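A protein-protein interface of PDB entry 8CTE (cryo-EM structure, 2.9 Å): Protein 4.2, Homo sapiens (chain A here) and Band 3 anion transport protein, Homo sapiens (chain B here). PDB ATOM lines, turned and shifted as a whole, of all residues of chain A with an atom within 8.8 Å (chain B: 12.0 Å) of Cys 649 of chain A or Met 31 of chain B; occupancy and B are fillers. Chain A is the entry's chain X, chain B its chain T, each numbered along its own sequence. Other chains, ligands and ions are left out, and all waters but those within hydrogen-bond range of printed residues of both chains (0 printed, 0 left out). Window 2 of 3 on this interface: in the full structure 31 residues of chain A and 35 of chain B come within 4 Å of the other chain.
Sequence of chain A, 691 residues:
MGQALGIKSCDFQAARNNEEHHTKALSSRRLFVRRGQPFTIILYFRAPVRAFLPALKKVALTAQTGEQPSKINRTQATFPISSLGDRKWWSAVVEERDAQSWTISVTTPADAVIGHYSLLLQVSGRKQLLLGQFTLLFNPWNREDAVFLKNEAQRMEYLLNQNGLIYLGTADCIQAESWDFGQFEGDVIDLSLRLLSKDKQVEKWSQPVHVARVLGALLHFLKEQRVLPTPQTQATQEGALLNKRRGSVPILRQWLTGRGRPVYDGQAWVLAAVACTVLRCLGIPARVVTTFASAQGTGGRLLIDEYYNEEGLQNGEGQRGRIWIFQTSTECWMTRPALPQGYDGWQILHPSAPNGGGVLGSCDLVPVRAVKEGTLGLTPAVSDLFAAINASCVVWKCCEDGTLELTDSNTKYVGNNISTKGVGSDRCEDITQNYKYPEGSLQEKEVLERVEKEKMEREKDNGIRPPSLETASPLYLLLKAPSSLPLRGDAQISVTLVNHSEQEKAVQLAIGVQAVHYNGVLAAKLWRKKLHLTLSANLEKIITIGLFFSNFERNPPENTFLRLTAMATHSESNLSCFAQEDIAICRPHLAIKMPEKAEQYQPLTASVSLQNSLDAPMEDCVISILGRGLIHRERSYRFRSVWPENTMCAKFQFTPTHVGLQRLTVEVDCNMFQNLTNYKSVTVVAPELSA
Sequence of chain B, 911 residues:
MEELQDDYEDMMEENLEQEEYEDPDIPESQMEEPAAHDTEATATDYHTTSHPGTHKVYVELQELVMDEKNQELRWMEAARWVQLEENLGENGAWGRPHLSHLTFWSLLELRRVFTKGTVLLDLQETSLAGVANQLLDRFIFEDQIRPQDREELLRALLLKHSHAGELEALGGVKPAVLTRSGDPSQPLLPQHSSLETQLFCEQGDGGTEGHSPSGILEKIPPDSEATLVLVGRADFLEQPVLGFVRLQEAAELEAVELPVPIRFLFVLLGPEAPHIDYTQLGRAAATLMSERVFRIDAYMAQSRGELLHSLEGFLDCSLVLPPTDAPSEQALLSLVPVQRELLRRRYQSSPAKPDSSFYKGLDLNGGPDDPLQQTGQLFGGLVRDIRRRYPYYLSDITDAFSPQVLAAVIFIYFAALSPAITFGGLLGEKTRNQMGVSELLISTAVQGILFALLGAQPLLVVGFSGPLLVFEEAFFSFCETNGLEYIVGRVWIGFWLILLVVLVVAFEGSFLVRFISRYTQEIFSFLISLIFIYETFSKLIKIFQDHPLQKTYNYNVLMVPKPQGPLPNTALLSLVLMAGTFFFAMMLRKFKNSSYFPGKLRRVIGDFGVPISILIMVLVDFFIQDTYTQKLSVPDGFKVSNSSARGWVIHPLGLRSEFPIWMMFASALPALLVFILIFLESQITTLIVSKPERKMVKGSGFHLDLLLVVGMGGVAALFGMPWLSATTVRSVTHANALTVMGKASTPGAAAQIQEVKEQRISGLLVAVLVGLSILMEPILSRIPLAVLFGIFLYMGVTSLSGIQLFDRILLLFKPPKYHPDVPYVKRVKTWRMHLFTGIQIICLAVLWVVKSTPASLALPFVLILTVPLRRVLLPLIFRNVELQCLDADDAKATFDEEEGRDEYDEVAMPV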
ATOM      1  N   ALA A 591      -5.563 -15.881  -2.274  1.00  0.00           N
ATOM      2  CA  ALA A 591      -5.270 -14.461  -2.144  1.00  0.00           C
ATOM      3  C   ALA A 591      -4.321 -14.226  -0.975  1.00  0.00           C
ATOM      4  O   ALA A 591      -4.561 -14.711   0.134  1.00  0.00           O
ATOM      5  CB  ALA A 591      -6.557 -13.658  -1.950  1.00  0.00           C
ATOM      6  N   ALA A 606       1.059 -11.104   7.271  1.00  0.00           N
ATOM      7  CA  ALA A 606       0.543 -11.486   5.964  1.00  0.00           C
ATOM      8  C   ALA A 606      -0.814 -12.154   6.131  1.00  0.00           C
ATOM      9  O   ALA A 606      -0.984 -13.018   6.998  1.00  0.00           O
ATOM     10  CB  ALA A 606       1.510 -12.426   5.240  1.00  0.00           C
ATOM     11  N   SER A 607      -1.770 -11.758   5.297  1.00  0.00           N
ATOM     12  CA  SER A 607      -3.126 -12.290   5.327  1.00  0.00           C
ATOM     13  C   SER A 607      -3.335 -13.215   4.136  1.00  0.00           C
ATOM     14  O   SER A 607      -3.022 -12.849   2.998  1.00  0.00           O
ATOM     15  CB  SER A 607      -4.155 -11.159   5.307  1.00  0.00           C
ATOM     16  OG  SER A 607      -5.305 -11.526   4.561  1.00  0.00           O
ATOM     17  N   VAL A 608      -3.869 -14.405   4.400  1.00  0.00           N
ATOM     18  CA  VAL A 608      -4.145 -15.399   3.369  1.00  0.00           C
ATOM     19  C   VAL A 608      -5.642 -15.672   3.356  1.00  0.00           C
ATOM     20  O   VAL A 608      -6.217 -16.061   4.379  1.00  0.00           O
ATOM     21  CB  VAL A 608      -3.354 -16.698   3.603  1.00  0.00           C
ATOM     22  CG1 VAL A 608      -3.774 -17.757   2.600  1.00  0.00           C
ATOM     23  CG2 VAL A 608      -1.862 -16.432   3.501  1.00  0.00           C
ATOM     24  N   SER A 609      -6.268 -15.471   2.200  1.00  0.00           N
ATOM     25  CA  SER A 609      -7.697 -15.682   2.026  1.00  0.00           C
ATOM     26  C   SER A 609      -7.942 -16.698   0.920  1.00  0.00           C
ATOM     27  O   SER A 609      -7.363 -16.602  -0.167  1.00  0.00           O
ATOM     28  CB  SER A 609      -8.416 -14.370   1.697  1.00  0.00           C
ATOM     29  OG  SER A 609      -8.293 -13.442   2.761  1.00  0.00           O
ATOM     30  N   LEU A 610      -8.806 -17.672   1.202  1.00  0.00           N
ATOM     31  CA  LEU A 610      -9.170 -18.698   0.233  1.00  0.00           C
ATOM     32  C   LEU A 610     -10.656 -18.986   0.367  1.00  0.00           C
ATOM     33  O   LEU A 610     -11.119 -19.378   1.443  1.00  0.00           O
ATOM     34  CB  LEU A 610      -8.352 -19.977   0.445  1.00  0.00           C
ATOM     35  CG  LEU A 610      -8.638 -21.148  -0.496  1.00  0.00           C
ATOM     36  CD1 LEU A 610      -8.275 -20.785  -1.922  1.00  0.00           C
ATOM     37  CD2 LEU A 610      -7.886 -22.393  -0.051  1.00  0.00           C
ATOM     38  N   GLN A 611     -11.399 -18.792  -0.718  1.00  0.00           N
ATOM     39  CA  GLN A 611     -12.836 -19.027  -0.725  1.00  0.00           C
ATOM     40  C   GLN A 611     -13.122 -20.403  -1.309  1.00  0.00           C
ATOM     41  O   GLN A 611     -12.630 -20.740  -2.390  1.00  0.00           O
ATOM     42  CB  GLN A 611     -13.553 -17.938  -1.527  1.00  0.00           C
ATOM     43  CG  GLN A 611     -15.033 -17.775  -1.200  1.00  0.00           C
ATOM     44  CD  GLN A 611     -15.924 -18.720  -1.982  1.00  0.00           C
ATOM     45  OE1 GLN A 611     -15.487 -19.350  -2.944  1.00  0.00           O
ATOM     46  NE2 GLN A 611     -17.183 -18.818  -1.574  1.00  0.00           N
ATOM     47  N   ILE A 623      -1.765 -25.531   5.607  1.00  0.00           N
ATOM     48  CA  ILE A 623      -1.214 -24.375   4.911  1.00  0.00           C
ATOM     49  C   ILE A 623       0.242 -24.209   5.333  1.00  0.00           C
ATOM     50  O   ILE A 623       0.572 -24.325   6.520  1.00  0.00           O
ATOM     51  CB  ILE A 623      -2.038 -23.100   5.179  1.00  0.00           C
ATOM     52  CG1 ILE A 623      -1.461 -21.905   4.415  1.00  0.00           C
ATOM     53  CG2 ILE A 623      -2.145 -22.803   6.669  1.00  0.00           C
ATOM     54  CD1 ILE A 623      -2.337 -20.668   4.460  1.00  0.00           C
ATOM     55  N   PHE A 639      -5.463 -25.473   9.589  1.00  0.00           N
ATOM     56  CA  PHE A 639      -6.631 -24.630   9.781  1.00  0.00           C
ATOM     57  C   PHE A 639      -7.900 -25.457   9.624  1.00  0.00           C
ATOM     58  O   PHE A 639      -7.887 -26.539   9.031  1.00  0.00           O
ATOM     59  CB  PHE A 639      -6.641 -23.427   8.815  1.00  0.00           C
ATOM     60  CG  PHE A 639      -6.622 -23.797   7.356  1.00  0.00           C
ATOM     61  CD1 PHE A 639      -5.429 -24.086   6.715  1.00  0.00           C
ATOM     62  CD2 PHE A 639      -7.792 -23.815   6.617  1.00  0.00           C
ATOM     63  CE1 PHE A 639      -5.406 -24.409   5.371  1.00  0.00           C
ATOM     64  CE2 PHE A 639      -7.776 -24.132   5.270  1.00  0.00           C
ATOM     65  CZ  PHE A 639      -6.580 -24.430   4.647  1.00  0.00           C
ATOM     66  N   ARG A 640      -8.994 -24.934  10.177  1.00  0.00           N
ATOM     67  CA  ARG A 640     -10.232 -25.694  10.286  1.00  0.00           C
ATOM     68  C   ARG A 640     -10.833 -25.968   8.913  1.00  0.00           C
ATOM     69  O   ARG A 640     -10.476 -25.336   7.914  1.00  0.00           O
ATOM     70  CB  ARG A 640     -11.243 -24.938  11.152  1.00  0.00           C
ATOM     71  CG  ARG A 640     -10.787 -24.698  12.580  1.00  0.00           C
ATOM     72  CD  ARG A 640     -11.802 -23.861  13.338  1.00  0.00           C
ATOM     73  NE  ARG A 640     -12.012 -22.567  12.703  1.00  0.00           N
ATOM     74  CZ  ARG A 640     -11.350 -21.462  13.019  1.00  0.00           C
ATOM     75  NH1 ARG A 640     -10.433 -21.455  13.972  1.00  0.00           N
ATOM     76  NH2 ARG A 640     -11.618 -20.336  12.363  1.00  0.00           N
ATOM     77  N   VAL A 642     -13.240 -25.903   5.824  1.00  0.00           N
ATOM     78  CA  VAL A 642     -13.962 -24.812   5.182  1.00  0.00           C
ATOM     79  C   VAL A 642     -15.129 -25.406   4.408  1.00  0.00           C
ATOM     80  O   VAL A 642     -14.929 -26.169   3.454  1.00  0.00           O
ATOM     81  CB  VAL A 642     -13.047 -23.991   4.259  1.00  0.00           C
ATOM     82  CG1 VAL A 642     -13.768 -22.749   3.765  1.00  0.00           C
ATOM     83  CG2 VAL A 642     -11.761 -23.619   4.981  1.00  0.00           C
ATOM     84  N   ASN A 646     -17.783 -20.716   1.898  1.00  0.00           N
ATOM     85  CA  ASN A 646     -17.155 -20.079   3.045  1.00  0.00           C
ATOM     86  C   ASN A 646     -15.745 -19.630   2.677  1.00  0.00           C
ATOM     87  O   ASN A 646     -15.128 -20.137   1.736  1.00  0.00           O
ATOM     88  CB  ASN A 646     -17.117 -21.025   4.253  1.00  0.00           C
ATOM     89  CG  ASN A 646     -18.496 -21.301   4.824  1.00  0.00           C
ATOM     90  OD1 ASN A 646     -19.512 -20.991   4.204  1.00  0.00           O
ATOM     91  ND2 ASN A 646     -18.535 -21.893   6.012  1.00  0.00           N
ATOM     92  N   THR A 647     -15.239 -18.665   3.438  1.00  0.00           N
ATOM     93  CA  THR A 647     -13.934 -18.064   3.191  1.00  0.00           C
ATOM     94  C   THR A 647     -13.014 -18.369   4.363  1.00  0.00           C
ATOM     95  O   THR A 647     -13.381 -18.142   5.522  1.00  0.00           O
ATOM     96  CB  THR A 647     -14.054 -16.551   2.988  1.00  0.00           C
ATOM     97  OG1 THR A 647     -14.920 -16.283   1.878  1.00  0.00           O
ATOM     98  CG2 THR A 647     -12.688 -15.936   2.718  1.00  0.00           C
ATOM     99  N   MET A 648     -11.824 -18.880   4.062  1.00  0.00           N
ATOM    100  CA  MET A 648     -10.804 -19.130   5.070  1.00  0.00           C
ATOM    101  C   MET A 648      -9.895 -17.913   5.167  1.00  0.00           C
ATOM    102  O   MET A 648      -9.343 -17.465   4.156  1.00  0.00           O
ATOM    103  CB  MET A 648      -9.994 -20.380   4.724  1.00  0.00           C
ATOM    104  CG  MET A 648      -8.838 -20.654   5.674  1.00  0.00           C
ATOM    105  SD  MET A 648      -7.245 -19.982   5.146  1.00  0.00           S
ATOM    106  CE  MET A 648      -6.917 -20.963   3.683  1.00  0.00           C
ATOM    107  N   CYS A 649      -9.743 -17.378   6.374  1.00  0.00           N
ATOM    108  CA  CYS A 649      -8.849 -16.258   6.629  1.00  0.00           C
ATOM    109  C   CYS A 649      -7.792 -16.686   7.637  1.00  0.00           C
ATOM    110  O   CYS A 649      -8.122 -17.055   8.769  1.00  0.00           O
ATOM    111  CB  CYS A 649      -9.621 -15.041   7.147  1.00  0.00           C
ATOM    112  SG  CYS A 649     -10.884 -14.422   6.010  1.00  0.00           S
ATOM    113  N   ALA A 650      -6.529 -16.636   7.224  1.00  0.00           N
ATOM    114  CA  ALA A 650      -5.407 -17.011   8.070  1.00  0.00           C
ATOM    115  C   ALA A 650      -4.425 -15.853   8.152  1.00  0.00           C
ATOM    116  O   ALA A 650      -4.112 -15.219   7.140  1.00  0.00           O
ATOM    117  CB  ALA A 650      -4.698 -18.263   7.540  1.00  0.00           C
ATOM    118  N   LYS A 651      -3.942 -15.583   9.359  1.00  0.00           N
ATOM    119  CA  LYS A 651      -3.011 -14.492   9.613  1.00  0.00           C
ATOM    120  C   LYS A 651      -1.685 -15.067  10.090  1.00  0.00           C
ATOM    121  O   LYS A 651      -1.656 -15.895  11.007  1.00  0.00           O
ATOM    122  CB  LYS A 651      -3.578 -13.524  10.654  1.00  0.00           C
ATOM    123  CG  LYS A 651      -3.279 -12.062  10.380  1.00  0.00           C
ATOM    124  CD  LYS A 651      -3.887 -11.616   9.061  1.00  0.00           C
ATOM    125  CE  LYS A 651      -3.708 -10.123   8.842  1.00  0.00           C
ATOM    126  NZ  LYS A 651      -4.359  -9.319   9.914  1.00  0.00           N
ATOM    127  N   PHE A 652      -0.594 -14.629   9.467  1.00  0.00           N
ATOM    128  CA  PHE A 652       0.747 -15.082   9.809  1.00  0.00           C
ATOM    129  C   PHE A 652       1.627 -13.876  10.094  1.00  0.00           C
ATOM    130  O   PHE A 652       1.647 -12.920   9.313  1.00  0.00           O
ATOM    131  CB  PHE A 652       1.354 -15.920   8.683  1.00  0.00           C
ATOM    132  CG  PHE A 652       0.495 -17.073   8.256  1.00  0.00           C
ATOM    133  CD1 PHE A 652       0.489 -18.253   8.980  1.00  0.00           C
ATOM    134  CD2 PHE A 652      -0.305 -16.978   7.130  1.00  0.00           C
ATOM    135  CE1 PHE A 652      -0.301 -19.317   8.590  1.00  0.00           C
ATOM    136  CE2 PHE A 652      -1.096 -18.040   6.734  1.00  0.00           C
ATOM    137  CZ  PHE A 652      -1.094 -19.212   7.467  1.00  0.00           C
ATOM    138  N   GLN B  30      -7.557 -12.479   9.219  1.00  0.00           N
ATOM    139  CA  GLN B  30      -7.166 -12.554  10.621  1.00  0.00           C
ATOM    140  C   GLN B  30      -8.234 -13.255  11.451  1.00  0.00           C
ATOM    141  O   GLN B  30      -8.239 -13.164  12.678  1.00  0.00           O
ATOM    142  CB  GLN B  30      -6.902 -11.155  11.181  1.00  0.00           C
ATOM    143  N   MET B  31      -9.144 -13.953  10.765  1.00  0.00           N
ATOM    144  CA  MET B  31     -10.223 -14.649  11.460  1.00  0.00           C
ATOM    145  C   MET B  31      -9.691 -15.807  12.296  1.00  0.00           C
ATOM    146  O   MET B  31     -10.174 -16.052  13.408  1.00  0.00           O
ATOM    147  CB  MET B  31     -11.259 -15.148  10.453  1.00  0.00           C
ATOM    148  N   GLU B  32      -8.700 -16.530  11.781  1.00  0.00           N
ATOM    149  CA  GLU B  32      -8.172 -17.719  12.434  1.00  0.00           C
ATOM    150  C   GLU B  32      -6.661 -17.613  12.572  1.00  0.00           C
ATOM    151  O   GLU B  32      -5.974 -17.208  11.629  1.00  0.00           O
ATOM    152  CB  GLU B  32      -8.540 -18.982  11.648  1.00  0.00           C
ATOM    153  CG  GLU B  32      -7.902 -20.256  12.179  1.00  0.00           C
ATOM    154  CD  GLU B  32      -8.309 -21.487  11.394  1.00  0.00           C
ATOM    155  OE1 GLU B  32      -8.829 -21.331  10.269  1.00  0.00           O
ATOM    156  OE2 GLU B  32      -8.111 -22.610  11.904  1.00  0.00           O
ATOM    157  N   GLU B  33      -6.150 -17.979  13.749  1.00  0.00           N
ATOM    158  CA  GLU B  33      -4.720 -18.166  13.933  1.00  0.00           C
ATOM    159  C   GLU B  33      -4.432 -19.657  13.882  1.00  0.00           C
ATOM    160  O   GLU B  33      -4.758 -20.373  14.842  1.00  0.00           O
ATOM    161  CB  GLU B  33      -4.256 -17.576  15.264  1.00  0.00           C
ATOM    162  CG  GLU B  33      -4.502 -16.081  15.408  1.00  0.00           C
ATOM    163  CD  GLU B  33      -3.963 -15.283  14.236  1.00  0.00           C
ATOM    164  OE1 GLU B  33      -4.748 -14.971  13.317  1.00  0.00           O
ATOM    165  OE2 GLU B  33      -2.752 -14.975  14.232  1.00  0.00           O
ATOM    166  N   PRO B  34      -3.843 -20.171  12.806  1.00  0.00           N
ATOM    167  CA  PRO B  34      -3.701 -21.623  12.665  1.00  0.00           C
ATOM    168  C   PRO B  34      -2.685 -22.203  13.636  1.00  0.00           C
ATOM    169  O   PRO B  34      -1.748 -21.531  14.074  1.00  0.00           O
ATOM    170  CB  PRO B  34      -3.240 -21.797  11.211  1.00  0.00           C
ATOM    171  CG  PRO B  34      -3.530 -20.485  10.539  1.00  0.00           C
ATOM    172  CD  PRO B  34      -3.388 -19.452  11.606  1.00  0.00           C
ATOM    173  N   ALA B  35      -2.885 -23.474  13.968  1.00  0.00           N
ATOM    174  CA  ALA B  35      -1.971 -24.209  14.827  1.00  0.00           C
ATOM    175  C   ALA B  35      -0.908 -24.909  13.989  1.00  0.00           C
ATOM    176  O   ALA B  35      -1.112 -25.197  12.808  1.00  0.00           O
ATOM    177  CB  ALA B  35      -2.728 -25.233  15.675  1.00  0.00           C
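The backbone NH (N) of Glu 32 of chain B lies within hydrogen-bond range of the backbone carbonyl oxygen (O) of Cys 649 of chain A, at 3.1 Å.
The side-chain carboxylate (OE2) of Glu 32 of chain B lies within salt-bridge range of the guanidinium group (NH1) of Arg 640 of chain A (3.3 Å).
The backbone carbonyl oxygen (O) of Glu 32 of chain B sits at hydrogen-bond distance from the backbone NH (N) of Lys 651 of chain A.
The backbone NH of Ala 606 of chain A is in hydrogen-bond range of the backbone carbonyl oxygen of Phe 652 of chain A, 2.8 Å away.
O of Ala 650 of chain A sits at hydrogen-bond distance from N of Val 608 of chain A (2.9 Å).
Among the printed residues, pairs that only touch across the chains: Phe 639 of chain A with Glu 32 of chain B (3.3 Å), Cys 649 of chain A with Gln 30 of chain B (3.9 Å), Cys 649 of chain A with Met 31 of chain B (3.7 Å), Ala 650 of chain A with Glu 32 of chain B (3.6 Å), Ala 650 of chain A with Pro 34 of chain B (3.9 Å), Lys 651 of chain A with Gln 30 of chain B (3.4 Å), Lys 651 of chain A with Glu 33 of chain B (3.2 Å) and Phe 652 of chain A with Pro 34 of chain B (3.9 Å).
No residue of chain B comes within 4 Å of Val 608 of chain A.
No residue of chain B comes within 4 Å of Ser 609 of chain A.
Of the printed residues of chain B, Phe 639 of chain A touches Glu 32.
No residue of chain B comes within 4 Å of Thr 647 of chain A.
Cys 649 of chain A touches three residues of chain B.
Of the printed residues of chain B, Ala 650 of chain A touches Glu 32 and Pro 34.
Gln 30 of chain B touches just these residues of chain A: Cys 649 (3.9 Å) and Lys 651 (3.4 Å).
Printed residues of chain A within 4 Å of Met 31 of chain B: Cys 649.
Of the printed residues of chain A, Pro 34 of chain B touches Ala 650 (3.9 Å) and Phe 652 (3.9 Å).
The nearest residue of chain B that does not touch Cys 649 of chain A is Glu 33 of chain B (5.4 Å).
The nearest residue of chain A that does not touch Met 31 of chain B is Arg 640 of chain A (4.6 Å).
The nearest printed residue of chain B that does not touch Phe 639 of chain A is Pro 34 of chain B (4.5 Å).
Of the 18 printed residues of chain A, 6 touch a printed residue of chain B.
Hydrophobic or aromatic side chains of chain A that line the printed part of chain B: Phe 639, Ala 650 and Phe 652.
Among the printed residues, 11 pairs touch across the chains.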
